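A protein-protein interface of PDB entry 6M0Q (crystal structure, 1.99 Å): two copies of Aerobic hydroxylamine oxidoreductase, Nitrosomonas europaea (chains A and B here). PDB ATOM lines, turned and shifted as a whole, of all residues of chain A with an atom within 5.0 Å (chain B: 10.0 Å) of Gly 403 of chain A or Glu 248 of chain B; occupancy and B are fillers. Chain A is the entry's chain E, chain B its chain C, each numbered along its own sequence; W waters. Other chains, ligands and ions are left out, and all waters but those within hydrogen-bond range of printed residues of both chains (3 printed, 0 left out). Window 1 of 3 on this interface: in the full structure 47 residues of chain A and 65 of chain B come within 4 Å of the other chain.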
ATOM      1  N   ASP A 398      15.337  24.441  -1.444  1.00  0.00           N
ATOM      2  CA  ASP A 398      16.468  24.997  -0.712  1.00  0.00           C
ATOM      3  C   ASP A 398      17.414  23.899  -0.223  1.00  0.00           C
ATOM      4  O   ASP A 398      18.647  24.017  -0.335  1.00  0.00           O
ATOM      5  CB  ASP A 398      15.977  25.830   0.461  1.00  0.00           C
ATOM      6  CG  ASP A 398      17.119  26.533   1.164  1.00  0.00           C
ATOM      7  OD1 ASP A 398      17.532  26.094   2.273  1.00  0.00           O
ATOM      8  OD2 ASP A 398      17.654  27.487   0.549  1.00  0.00           O
ATOM      9  N   LEU A 399      16.856  22.835   0.359  1.00  0.00           N
ATOM     10  CA  LEU A 399      17.664  21.670   0.718  1.00  0.00           C
ATOM     11  C   LEU A 399      18.463  21.171  -0.484  1.00  0.00           C
ATOM     12  O   LEU A 399      19.681  20.950  -0.391  1.00  0.00           O
ATOM     13  CB  LEU A 399      16.764  20.564   1.275  1.00  0.00           C
ATOM     14  CG  LEU A 399      17.408  19.290   1.844  1.00  0.00           C
ATOM     15  CD1 LEU A 399      16.432  18.592   2.790  1.00  0.00           C
ATOM     16  CD2 LEU A 399      17.760  18.327   0.771  1.00  0.00           C
ATOM     17  N   MET A 400      17.792  20.996  -1.626  1.00  0.00           N
ATOM     18  CA  MET A 400      18.481  20.519  -2.828  1.00  0.00           C
ATOM     19  C   MET A 400      19.676  21.397  -3.174  1.00  0.00           C
ATOM     20  O   MET A 400      20.777  20.889  -3.415  1.00  0.00           O
ATOM     21  CB  MET A 400      17.514  20.457  -4.014  1.00  0.00           C
ATOM     22  CG  MET A 400      18.193  20.102  -5.306  1.00  0.00           C
ATOM     23  SD  MET A 400      17.119  20.409  -6.714  1.00  0.00           S
ATOM     24  CE  MET A 400      17.174  22.195  -6.778  1.00  0.00           C
ATOM     25  N   ASP A 401      19.480  22.721  -3.191  1.00  0.00           N
ATOM     26  CA  ASP A 401      20.564  23.626  -3.581  1.00  0.00           C
ATOM     27  C   ASP A 401      21.717  23.575  -2.585  1.00  0.00           C
ATOM     28  O   ASP A 401      22.885  23.527  -2.981  1.00  0.00           O
ATOM     29  CB  ASP A 401      20.062  25.069  -3.713  1.00  0.00           C
ATOM     30  CG  ASP A 401      19.254  25.318  -4.988  1.00  0.00           C
ATOM     31  OD1 ASP A 401      19.268  24.474  -5.914  1.00  0.00           O
ATOM     32  OD2 ASP A 401      18.576  26.373  -5.048  1.00  0.00           O
ATOM     33  N   LYS A 402      21.410  23.606  -1.282  1.00  0.00           N
ATOM     34  CA  LYS A 402      22.475  23.622  -0.285  1.00  0.00           C
ATOM     35  C   LYS A 402      23.145  22.268  -0.188  1.00  0.00           C
ATOM     36  O   LYS A 402      24.371  22.181  -0.025  1.00  0.00           O
ATOM     37  CB  LYS A 402      21.924  24.047   1.078  1.00  0.00           C
ATOM     38  CG  LYS A 402      21.641  25.557   1.132  1.00  0.00           C
ATOM     39  CD  LYS A 402      20.796  25.984   2.325  1.00  0.00           C
ATOM     40  CE  LYS A 402      20.537  27.504   2.247  1.00  0.00           C
ATOM     41  NZ  LYS A 402      19.422  27.984   3.115  1.00  0.00           N
ATOM     42  N   GLY A 403      22.351  21.202  -0.270  1.00  0.00           N
ATOM     43  CA  GLY A 403      22.924  19.868  -0.291  1.00  0.00           C
ATOM     44  C   GLY A 403      23.892  19.681  -1.440  1.00  0.00           C
ATOM     45  O   GLY A 403      24.953  19.064  -1.282  1.00  0.00           O
ATOM     46  N   THR A 404      23.547  20.221  -2.612  1.00  0.00           N
ATOM     47  CA  THR A 404      24.430  20.067  -3.760  1.00  0.00           C
ATOM     48  C   THR A 404      25.744  20.799  -3.513  1.00  0.00           C
ATOM     49  O   THR A 404      26.825  20.265  -3.797  1.00  0.00           O
ATOM     50  CB  THR A 404      23.715  20.571  -5.017  1.00  0.00           C
ATOM     51  OG1 THR A 404      22.541  19.777  -5.222  1.00  0.00           O
ATOM     52  CG2 THR A 404      24.597  20.457  -6.239  1.00  0.00           C
ATOM     53  N   LEU A 405      25.662  22.012  -2.951  1.00  0.00           N
ATOM     54  CA  LEU A 405      26.868  22.775  -2.639  1.00  0.00           C
ATOM     55  C   LEU A 405      27.699  22.080  -1.578  1.00  0.00           C
ATOM     56  O   LEU A 405      28.936  22.136  -1.616  1.00  0.00           O
ATOM     57  CB  LEU A 405      26.499  24.176  -2.162  1.00  0.00           C
ATOM     58  CG  LEU A 405      25.914  25.126  -3.202  1.00  0.00           C
ATOM     59  CD1 LEU A 405      25.367  26.334  -2.495  1.00  0.00           C
ATOM     60  CD2 LEU A 405      26.971  25.545  -4.212  1.00  0.00           C
ATOM     61  N   GLU A 406      27.042  21.460  -0.595  1.00  0.00           N
ATOM     62  CA  GLU A 406      27.795  20.734   0.413  1.00  0.00           C
ATOM     63  C   GLU A 406      28.586  19.605  -0.221  1.00  0.00           C
ATOM     64  O   GLU A 406      29.754  19.390   0.118  1.00  0.00           O
ATOM     65  CB  GLU A 406      26.846  20.223   1.498  1.00  0.00           C
ATOM     66  CG  GLU A 406      26.365  21.374   2.375  1.00  0.00           C
ATOM     67  CD  GLU A 406      25.043  21.121   3.076  1.00  0.00           C
ATOM     68  OE1 GLU A 406      24.588  19.966   3.182  1.00  0.00           O
ATOM     69  OE2 GLU A 406      24.449  22.122   3.510  1.00  0.00           O
ATOM     70  N   GLY A 407      27.979  18.894  -1.171  1.00  0.00           N
ATOM     71  CA  GLY A 407      28.727  17.910  -1.929  1.00  0.00           C
ATOM     72  C   GLY A 407      29.849  18.530  -2.735  1.00  0.00           C
ATOM     73  O   GLY A 407      30.966  18.015  -2.758  1.00  0.00           O
ATOM     74  N   MET A 477      24.917  12.505  -6.374  1.00  0.00           N
ATOM     75  CA  MET A 477      24.448  13.203  -5.182  1.00  0.00           C
ATOM     76  C   MET A 477      23.433  14.270  -5.550  1.00  0.00           C
ATOM     77  O   MET A 477      22.347  14.363  -4.955  1.00  0.00           O
ATOM     78  CB  MET A 477      25.614  13.838  -4.442  1.00  0.00           C
ATOM     79  CG  MET A 477      25.162  14.385  -3.089  1.00  0.00           C
ATOM     80  SD  MET A 477      26.485  15.143  -2.174  1.00  0.00           S
ATOM     81  CE  MET A 477      25.550  15.841  -0.803  1.00  0.00           C
ATOM     82  N   LEU A 481      19.388  14.396  -4.674  1.00  0.00           N
ATOM     83  CA  LEU A 481      18.730  15.534  -4.038  1.00  0.00           C
ATOM     84  C   LEU A 481      17.604  16.050  -4.903  1.00  0.00           C
ATOM     85  O   LEU A 481      16.502  16.315  -4.419  1.00  0.00           O
ATOM     86  CB  LEU A 481      19.735  16.655  -3.785  1.00  0.00           C
ATOM     87  CG  LEU A 481      20.662  16.375  -2.618  1.00  0.00           C
ATOM     88  CD1 LEU A 481      21.913  17.180  -2.822  1.00  0.00           C
ATOM     89  CD2 LEU A 481      19.945  16.796  -1.374  1.00  0.00           C
ATOM     90  N   TRP A 489      21.502  10.618  -1.737  1.00  0.00           N
ATOM     91  CA  TRP A 489      22.525  11.614  -1.521  1.00  0.00           C
ATOM     92  C   TRP A 489      23.240  11.440  -0.202  1.00  0.00           C
ATOM     93  O   TRP A 489      24.152  12.223   0.091  1.00  0.00           O
ATOM     94  CB  TRP A 489      21.962  13.039  -1.626  1.00  0.00           C
ATOM     95  CG  TRP A 489      21.099  13.548  -0.483  1.00  0.00           C
ATOM     96  CD1 TRP A 489      21.525  14.114   0.696  1.00  0.00           C
ATOM     97  CD2 TRP A 489      19.674  13.632  -0.467  1.00  0.00           C
ATOM     98  NE1 TRP A 489      20.452  14.532   1.442  1.00  0.00           N
ATOM     99  CE2 TRP A 489      19.302  14.258   0.749  1.00  0.00           C
ATOM    100  CE3 TRP A 489      18.672  13.269  -1.372  1.00  0.00           C
ATOM    101  CZ2 TRP A 489      17.985  14.520   1.076  1.00  0.00           C
ATOM    102  CZ3 TRP A 489      17.354  13.524  -1.033  1.00  0.00           C
ATOM    103  CH2 TRP A 489      17.026  14.138   0.192  1.00  0.00           C
ATOM    104  N   TRP B  73      22.678  21.346  16.868  1.00  0.00           N
ATOM    105  CA  TRP B  73      22.085  21.423  15.544  1.00  0.00           C
ATOM    106  C   TRP B  73      20.827  22.251  15.633  1.00  0.00           C
ATOM    107  O   TRP B  73      20.208  22.346  16.697  1.00  0.00           O
ATOM    108  CB  TRP B  73      21.756  20.030  14.972  1.00  0.00           C
ATOM    109  CG  TRP B  73      20.753  19.229  15.805  1.00  0.00           C
ATOM    110  CD1 TRP B  73      21.032  18.386  16.837  1.00  0.00           C
ATOM    111  CD2 TRP B  73      19.333  19.196  15.634  1.00  0.00           C
ATOM    112  NE1 TRP B  73      19.871  17.824  17.320  1.00  0.00           N
ATOM    113  CE2 TRP B  73      18.814  18.310  16.600  1.00  0.00           C
ATOM    114  CE3 TRP B  73      18.448  19.827  14.749  1.00  0.00           C
ATOM    115  CZ2 TRP B  73      17.454  18.045  16.716  1.00  0.00           C
ATOM    116  CZ3 TRP B  73      17.094  19.550  14.852  1.00  0.00           C
ATOM    117  CH2 TRP B  73      16.611  18.662  15.830  1.00  0.00           C
ATOM    118  N   GLU B  74      20.466  22.864  14.512  1.00  0.00           N
ATOM    119  CA  GLU B  74      19.254  23.651  14.397  1.00  0.00           C
ATOM    120  C   GLU B  74      18.427  23.134  13.226  1.00  0.00           C
ATOM    121  O   GLU B  74      18.978  22.599  12.262  1.00  0.00           O
ATOM    122  CB  GLU B  74      19.566  25.141  14.196  1.00  0.00           C
ATOM    123  CG  GLU B  74      20.261  25.789  15.402  1.00  0.00           C
ATOM    124  CD  GLU B  74      21.724  25.356  15.540  1.00  0.00           C
ATOM    125  OE1 GLU B  74      22.438  25.356  14.516  1.00  0.00           O
ATOM    126  OE2 GLU B  74      22.151  25.000  16.664  1.00  0.00           O
ATOM    127  N   PRO B  75      17.103  23.255  13.298  1.00  0.00           N
ATOM    128  CA  PRO B  75      16.263  22.848  12.172  1.00  0.00           C
ATOM    129  C   PRO B  75      16.629  23.611  10.914  1.00  0.00           C
ATOM    130  O   PRO B  75      17.184  24.707  10.952  1.00  0.00           O
ATOM    131  CB  PRO B  75      14.852  23.211  12.632  1.00  0.00           C
ATOM    132  CG  PRO B  75      15.086  24.347  13.616  1.00  0.00           C
ATOM    133  CD  PRO B  75      16.335  23.977  14.334  1.00  0.00           C
ATOM    134  N   ILE B  76      16.324  23.008   9.784  1.00  0.00           N
ATOM    135  CA  ILE B  76      16.387  23.766   8.549  1.00  0.00           C
ATOM    136  C   ILE B  76      14.953  23.892   8.065  1.00  0.00           C
ATOM    137  O   ILE B  76      14.024  23.410   8.726  1.00  0.00           O
ATOM    138  CB  ILE B  76      17.308  23.100   7.522  1.00  0.00           C
ATOM    139  CG1 ILE B  76      16.806  21.687   7.198  1.00  0.00           C
ATOM    140  CG2 ILE B  76      18.734  23.102   8.043  1.00  0.00           C
ATOM    141  CD1 ILE B  76      17.456  21.086   5.956  1.00  0.00           C
ATOM    142  N   ALA B  77      14.755  24.534   6.918  1.00  0.00           N
ATOM    143  CA  ALA B  77      13.401  24.897   6.506  1.00  0.00           C
ATOM    144  C   ALA B  77      12.463  23.680   6.477  1.00  0.00           C
ATOM    145  O   ALA B  77      11.332  23.752   6.939  1.00  0.00           O
ATOM    146  CB  ALA B  77      13.441  25.602   5.145  1.00  0.00           C
ATOM    147  N   ILE B  78      12.908  22.552   5.917  1.00  0.00           N
ATOM    148  CA  ILE B  78      11.991  21.421   5.804  1.00  0.00           C
ATOM    149  C   ILE B  78      11.804  20.691   7.126  1.00  0.00           C
ATOM    150  O   ILE B  78      10.857  19.904   7.257  1.00  0.00           O
ATOM    151  CB  ILE B  78      12.477  20.471   4.687  1.00  0.00           C
ATOM    152  CG1 ILE B  78      11.318  19.624   4.174  1.00  0.00           C
ATOM    153  CG2 ILE B  78      13.658  19.645   5.163  1.00  0.00           C
ATOM    154  CD1 ILE B  78      11.601  18.901   2.881  1.00  0.00           C
ATOM    155  N   SER B  79      12.637  20.972   8.136  1.00  0.00           N
ATOM    156  CA  SER B  79      12.479  20.310   9.432  1.00  0.00           C
ATOM    157  C   SER B  79      11.084  20.499  10.018  1.00  0.00           C
ATOM    158  O   SER B  79      10.685  19.718  10.894  1.00  0.00           O
ATOM    159  CB  SER B  79      13.523  20.829  10.436  1.00  0.00           C
ATOM    160  OG  SER B  79      14.829  20.751   9.888  1.00  0.00           O
ATOM    161  N   MET B  82       9.300  17.541   9.001  1.00  0.00           N
ATOM    162  CA  MET B  82       9.887  16.301   9.492  1.00  0.00           C
ATOM    163  C   MET B  82       9.594  16.093  10.965  1.00  0.00           C
ATOM    164  O   MET B  82       9.331  14.970  11.389  1.00  0.00           O
ATOM    165  CB  MET B  82      11.390  16.313   9.268  1.00  0.00           C
ATOM    166  CG  MET B  82      11.776  16.645   7.842  1.00  0.00           C
ATOM    167  SD  MET B  82      11.514  15.188   6.822  1.00  0.00           S
ATOM    168  CE  MET B  82       9.898  15.424   6.106  1.00  0.00           C
ATOM    169  N   VAL B 240      26.843  11.762  14.709  1.00  0.00           N
ATOM    170  CA  VAL B 240      27.298  12.448  13.500  1.00  0.00           C
ATOM    171  C   VAL B 240      26.160  13.243  12.885  1.00  0.00           C
ATOM    172  O   VAL B 240      26.379  14.328  12.338  1.00  0.00           O
ATOM    173  CB  VAL B 240      27.924  11.467  12.485  1.00  0.00           C
ATOM    174  CG1 VAL B 240      26.867  10.599  11.823  1.00  0.00           C
ATOM    175  CG2 VAL B 240      28.739  12.256  11.426  1.00  0.00           C
ATOM    176  N   TRP B 241      24.930  12.739  12.981  1.00  0.00           N
ATOM    177  CA  TRP B 241      23.791  13.505  12.491  1.00  0.00           C
ATOM    178  C   TRP B 241      23.682  14.840  13.220  1.00  0.00           C
ATOM    179  O   TRP B 241      23.380  15.871  12.615  1.00  0.00           O
ATOM    180  CB  TRP B 241      22.501  12.699  12.656  1.00  0.00           C
ATOM    181  CG  TRP B 241      21.316  13.438  12.114  1.00  0.00           C
ATOM    182  CD1 TRP B 241      20.820  13.358  10.861  1.00  0.00           C
ATOM    183  CD2 TRP B 241      20.512  14.403  12.809  1.00  0.00           C
ATOM    184  NE1 TRP B 241      19.727  14.185  10.729  1.00  0.00           N
ATOM    185  CE2 TRP B 241      19.526  14.850  11.906  1.00  0.00           C
ATOM    186  CE3 TRP B 241      20.523  14.922  14.112  1.00  0.00           C
ATOM    187  CZ2 TRP B 241      18.560  15.790  12.259  1.00  0.00           C
ATOM    188  CZ3 TRP B 241      19.564  15.848  14.460  1.00  0.00           C
ATOM    189  CH2 TRP B 241      18.594  16.276  13.535  1.00  0.00           C
ATOM    190  N   MET B 244      27.486  16.943  12.366  1.00  0.00           N
ATOM    191  CA  MET B 244      28.075  17.312  11.094  1.00  0.00           C
ATOM    192  C   MET B 244      27.529  18.660  10.656  1.00  0.00           C
ATOM    193  O   MET B 244      26.382  18.993  10.951  1.00  0.00           O
ATOM    194  CB  MET B 244      27.774  16.261  10.031  1.00  0.00           C
ATOM    195  CG  MET B 244      26.277  16.010   9.803  1.00  0.00           C
ATOM    196  SD  MET B 244      25.971  14.539   8.761  1.00  0.00           S
ATOM    197  CE  MET B 244      26.799  15.043   7.240  1.00  0.00           C
ATOM    198  N   PRO B 245      28.339  19.451   9.950  1.00  0.00           N
ATOM    199  CA  PRO B 245      27.862  20.760   9.482  1.00  0.00           C
ATOM    200  C   PRO B 245      26.983  20.680   8.250  1.00  0.00           C
ATOM    201  O   PRO B 245      26.187  21.590   8.027  1.00  0.00           O
ATOM    202  CB  PRO B 245      29.160  21.516   9.178  1.00  0.00           C
ATOM    203  CG  PRO B 245      30.114  20.414   8.719  1.00  0.00           C
ATOM    204  CD  PRO B 245      29.756  19.213   9.615  1.00  0.00           C
ATOM    205  N   GLN B 246      27.085  19.632   7.450  1.00  0.00           N
ATOM    206  CA  GLN B 246      26.292  19.541   6.220  1.00  0.00           C
ATOM    207  C   GLN B 246      24.866  19.144   6.599  1.00  0.00           C
ATOM    208  O   GLN B 246      24.476  17.970   6.579  1.00  0.00           O
ATOM    209  CB  GLN B 246      26.917  18.552   5.252  1.00  0.00           C
ATOM    210  CG  GLN B 246      28.332  18.907   4.815  1.00  0.00           C
ATOM    211  CD  GLN B 246      29.372  18.469   5.811  1.00  0.00           C
ATOM    212  OE1 GLN B 246      29.046  17.849   6.827  1.00  0.00           O
ATOM    213  NE2 GLN B 246      30.637  18.732   5.507  1.00  0.00           N
ATOM    214  N   ARG B 247      24.072  20.155   6.955  1.00  0.00           N
ATOM    215  CA  ARG B 247      22.750  19.868   7.499  1.00  0.00           C
ATOM    216  C   ARG B 247      21.815  19.314   6.442  1.00  0.00           C
ATOM    217  O   ARG B 247      20.905  18.528   6.749  1.00  0.00           O
ATOM    218  CB  ARG B 247      22.147  21.130   8.107  1.00  0.00           C
ATOM    219  CG  ARG B 247      22.976  21.751   9.234  1.00  0.00           C
ATOM    220  CD  ARG B 247      23.416  20.727  10.247  1.00  0.00           C
ATOM    221  NE  ARG B 247      22.280  19.964  10.771  1.00  0.00           N
ATOM    222  CZ  ARG B 247      22.413  18.761  11.298  1.00  0.00           C
ATOM    223  NH1 ARG B 247      23.624  18.220  11.345  1.00  0.00           N
ATOM    224  NH2 ARG B 247      21.357  18.085  11.731  1.00  0.00           N
ATOM    225  N   GLU B 248      21.994  19.734   5.196  1.00  0.00           N
ATOM    226  CA  GLU B 248      21.136  19.211   4.151  1.00  0.00           C
ATOM    227  C   GLU B 248      21.445  17.749   3.856  1.00  0.00           C
ATOM    228  O   GLU B 248      20.530  16.977   3.545  1.00  0.00           O
ATOM    229  CB  GLU B 248      21.262  20.086   2.918  1.00  0.00           C
ATOM    230  CG  GLU B 248      20.455  21.369   3.009  1.00  0.00           C
ATOM    231  CD  GLU B 248      20.977  22.386   4.039  1.00  0.00           C
ATOM    232  OE1 GLU B 248      22.137  22.296   4.474  1.00  0.00           O
ATOM    233  OE2 GLU B 248      20.216  23.301   4.411  1.00  0.00           O
ATOM    234  N   VAL B 249      22.711  17.333   3.971  1.00  0.00           N
ATOM    235  CA  VAL B 249      23.007  15.901   3.911  1.00  0.00           C
ATOM    236  C   VAL B 249      22.317  15.180   5.056  1.00  0.00           C
ATOM    237  O   VAL B 249      21.641  14.161   4.864  1.00  0.00           O
ATOM    238  CB  VAL B 249      24.525  15.649   3.938  1.00  0.00           C
ATOM    239  CG1 VAL B 249      24.795  14.144   4.017  1.00  0.00           C
ATOM    240  CG2 VAL B 249      25.203  16.259   2.714  1.00  0.00           C
ATOM    241  N   ALA B 250      22.461  15.721   6.268  1.00  0.00           N
ATOM    242  CA  ALA B 250      21.894  15.089   7.454  1.00  0.00           C
ATOM    243  C   ALA B 250      20.385  14.970   7.364  1.00  0.00           C
ATOM    244  O   ALA B 250      19.804  14.005   7.885  1.00  0.00           O
ATOM    245  CB  ALA B 250      22.268  15.890   8.698  1.00  0.00           C
ATOM    246  N   GLU B 251      19.727  15.939   6.730  1.00  0.00           N
ATOM    247  CA  GLU B 251      18.286  15.844   6.663  1.00  0.00           C
ATOM    248  C   GLU B 251      17.846  14.761   5.709  1.00  0.00           C
ATOM    249  O   GLU B 251      16.699  14.305   5.806  1.00  0.00           O
ATOM    250  CB  GLU B 251      17.670  17.186   6.287  1.00  0.00           C
ATOM    251  CG  GLU B 251      16.289  17.379   6.919  1.00  0.00           C
ATOM    252  CD  GLU B 251      16.273  17.321   8.471  1.00  0.00           C
ATOM    253  OE1 GLU B 251      17.334  17.267   9.133  1.00  0.00           O
ATOM    254  OE2 GLU B 251      15.159  17.348   9.029  1.00  0.00           O
ATOM    255  N   GLY B 252      18.733  14.328   4.803  1.00  0.00           N
ATOM    256  CA  GLY B 252      18.461  13.115   4.053  1.00  0.00           C
ATOM    257  C   GLY B 252      18.231  11.942   4.977  1.00  0.00           C
ATOM    258  O   GLY B 252      17.304  11.143   4.780  1.00  0.00           O
ATOM    259  N   CYS B 253      19.065  11.825   6.009  1.00  0.00           N
ATOM    260  CA  CYS B 253      18.836  10.799   7.022  1.00  0.00           C
ATOM    261  C   CYS B 253      17.473  10.968   7.656  1.00  0.00           C
ATOM    262  O   CYS B 253      16.725   9.997   7.844  1.00  0.00           O
ATOM    263  CB  CYS B 253      19.921  10.885   8.084  1.00  0.00           C
ATOM    264  SG  CYS B 253      21.545  10.767   7.397  1.00  0.00           S
ATOM    265  N   THR B 254      17.130  12.205   7.987  1.00  0.00           N
ATOM    266  CA  THR B 254      15.879  12.475   8.664  1.00  0.00           C
ATOM    267  C   THR B 254      14.689  12.004   7.837  1.00  0.00           C
ATOM    268  O   THR B 254      13.732  11.433   8.383  1.00  0.00           O
ATOM    269  CB  THR B 254      15.793  13.970   8.983  1.00  0.00           C
ATOM    270  OG1 THR B 254      16.849  14.305   9.895  1.00  0.00           O
ATOM    271  CG2 THR B 254      14.464  14.314   9.649  1.00  0.00           C
ATOM    272  N   MET B 255      14.744  12.200   6.519  1.00  0.00           N
ATOM    273  CA  MET B 255      13.618  11.821   5.673  1.00  0.00           C
ATOM    274  C   MET B 255      13.328  10.334   5.711  1.00  0.00           C
ATOM    275  O   MET B 255      12.218   9.929   5.349  1.00  0.00           O
ATOM    276  CB  MET B 255      13.869  12.264   4.222  1.00  0.00           C
ATOM    277  CG  MET B 255      13.840  13.764   4.147  1.00  0.00           C
ATOM    278  SD  MET B 255      14.104  14.365   2.490  1.00  0.00           S
ATOM    279  CE  MET B 255      12.663  13.710   1.638  1.00  0.00           C
ATOM    280  N   PHE B 452      30.063   9.559   7.548  1.00  0.00           N
ATOM    281  CA  PHE B 452      29.407  10.800   7.161  1.00  0.00           C
ATOM    282  C   PHE B 452      30.248  12.028   7.437  1.00  0.00           C
ATOM    283  O   PHE B 452      29.855  13.142   7.048  1.00  0.00           O
ATOM    284  CB  PHE B 452      28.062  10.934   7.883  1.00  0.00           C
ATOM    285  CG  PHE B 452      27.001  10.096   7.282  1.00  0.00           C
ATOM    286  CD1 PHE B 452      26.178  10.620   6.307  1.00  0.00           C
ATOM    287  CD2 PHE B 452      26.840   8.764   7.677  1.00  0.00           C
ATOM    288  CE1 PHE B 452      25.191   9.835   5.714  1.00  0.00           C
ATOM    289  CE2 PHE B 452      25.873   7.965   7.089  1.00  0.00           C
ATOM    290  CZ  PHE B 452      25.043   8.508   6.100  1.00  0.00           C
HETATM  291  O   HOH W   1      17.657  23.822   3.671  1.00  0.00           O
HETATM  292  O   HOH W   2      16.807  26.096   5.325  1.00  0.00           O
HETATM  293  O   HOH W   3      30.981  19.640   2.765  1.00  0.00           O
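Of the 13 printed residues of chain A, 6 touch a printed residue of chain B.
Printed residues of chain A that touch a printed residue of chain B: Leu 399, Lys 402, Gly 403, Glu 406, Met 477 and Trp 489.
Hydrophobic or aromatic side chains of chain A within 4 Å of the printed part of chain B: Leu 399, Met 477 and Trp 489.
Among the printed residues, 14 pairs touch across the chains.
Among the printed residues, no Asp or Glu carboxylate lies within 4 Å of a Lys or Arg side-chain nitrogen of the other chain.
The backbone NH of Glu 248 of chain B lies within hydrogen-bond range of the side-chain carboxylate of Glu 406 of chain A.
The backbone carbonyl oxygen of Glu 248 of chain B lies within hydrogen-bond range of the indole nitrogen of Trp 489 of chain A (3.2 Å).
The side-chain carboxylate (OE1) of Glu 406 of chain A sits at hydrogen-bond distance from the backbone NH (N) of Val 249 of chain B (3.3 Å).
Water W1 lies within hydrogen-bond range of OD1 of Asp 398 of chain A and OE2 of Glu 248 of chain B.
Water W3 bridges NE2 of Gln 246 of chain B (2.9 Å) and O of Glu 406 of chain A (2.9 Å).
Water W2 lies within hydrogen-bond range of the backbone NH (N) of Ala 77 of chain B and the side-chain carboxylate (OD1) of Asp 398 of chain A.
The guanidinium group (NH1) of Arg 247 of chain B lies within hydrogen-bond range of the backbone carbonyl oxygen (O) of Trp 241 of chain B, at 2.7 Å.
The backbone carbonyl oxygen (O) of Met 244 of chain B is in hydrogen-bond range of the guanidinium group (NH1) of Arg 247 of chain B, at 2.9 Å.
The side-chain carboxylate (OE1) of Glu 251 of chain B is in hydrogen-bond range of the side-chain hydroxyl (OG1) of Thr 254 of chain B (3.1 Å).
NZ of Lys 402 of chain A is in salt-bridge range of OD1 of Asp 398 of chain A, 2.8 Å away.
Printed residues of chain A within 4 Å of Glu 248 of chain B: Leu 399, Lys 402, Gly 403, Glu 406 and Trp 489.
Of chain B, only Glu 248 comes within 4 Å of Lys 402 of chain A.
No residue of chain B comes within 4 Å of Thr 404 of chain A.
Of chain B, only Gln 246, Arg 247, Glu 248 and Val 249 come within 4 Å of Glu 406 of chain A.
Of the printed residues of chain B, Trp 489 of chain A touches Glu 248, Val 249, Gly 252 and Met 255.
Printed residues of chain A within 4 Å of Met 255 of chain B: Trp 489 (3.7 Å).
Of the printed residues of chain A, Arg 247 of chain B touches Glu 406 (3.8 Å).
Of the printed residues of chain B, Met 477 of chain A touches Val 249 (3.6 Å).
Of the printed residues of chain A, Gln 246 of chain B touches Glu 406 (3.4 Å).
Ala 250 of chain B touches none of the printed residues of chain A.
The nearest residue of chain A that does not touch Glu 248 of chain B is Asp 398 of chain A (4.4 Å).
No position is printed for both chains.
Leu 399 of chain A touches Ile 78 of chain B.
Leu 399 of chain A touches Glu 248 of chain B (O to CG, 3.5 Å).
Glu 251 of chain B touches Leu 399 of chain A (CB to CD1, 3.97 Å).
Lys 402 of chain A touches Glu 248 of chain B (CD to OE2, 3.4 Å).
N of Gly 403 of chain A touches CB of Glu 248 of chain B, 3.5 Å away.
Glu 406 of chain A touches Gln 246 of chain B (OE1 to CB, 3.4 Å).
Glu 406 of chain A touches Arg 247 of chain B.
Met 477 of chain A touches Val 249 of chain B (CE to CG2, 3.6 Å).
Trp 489 of chain A touches Val 249 of chain B (NE1 to O, 3.6 Å).
Met 255 of chain B touches Trp 489 of chain A.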
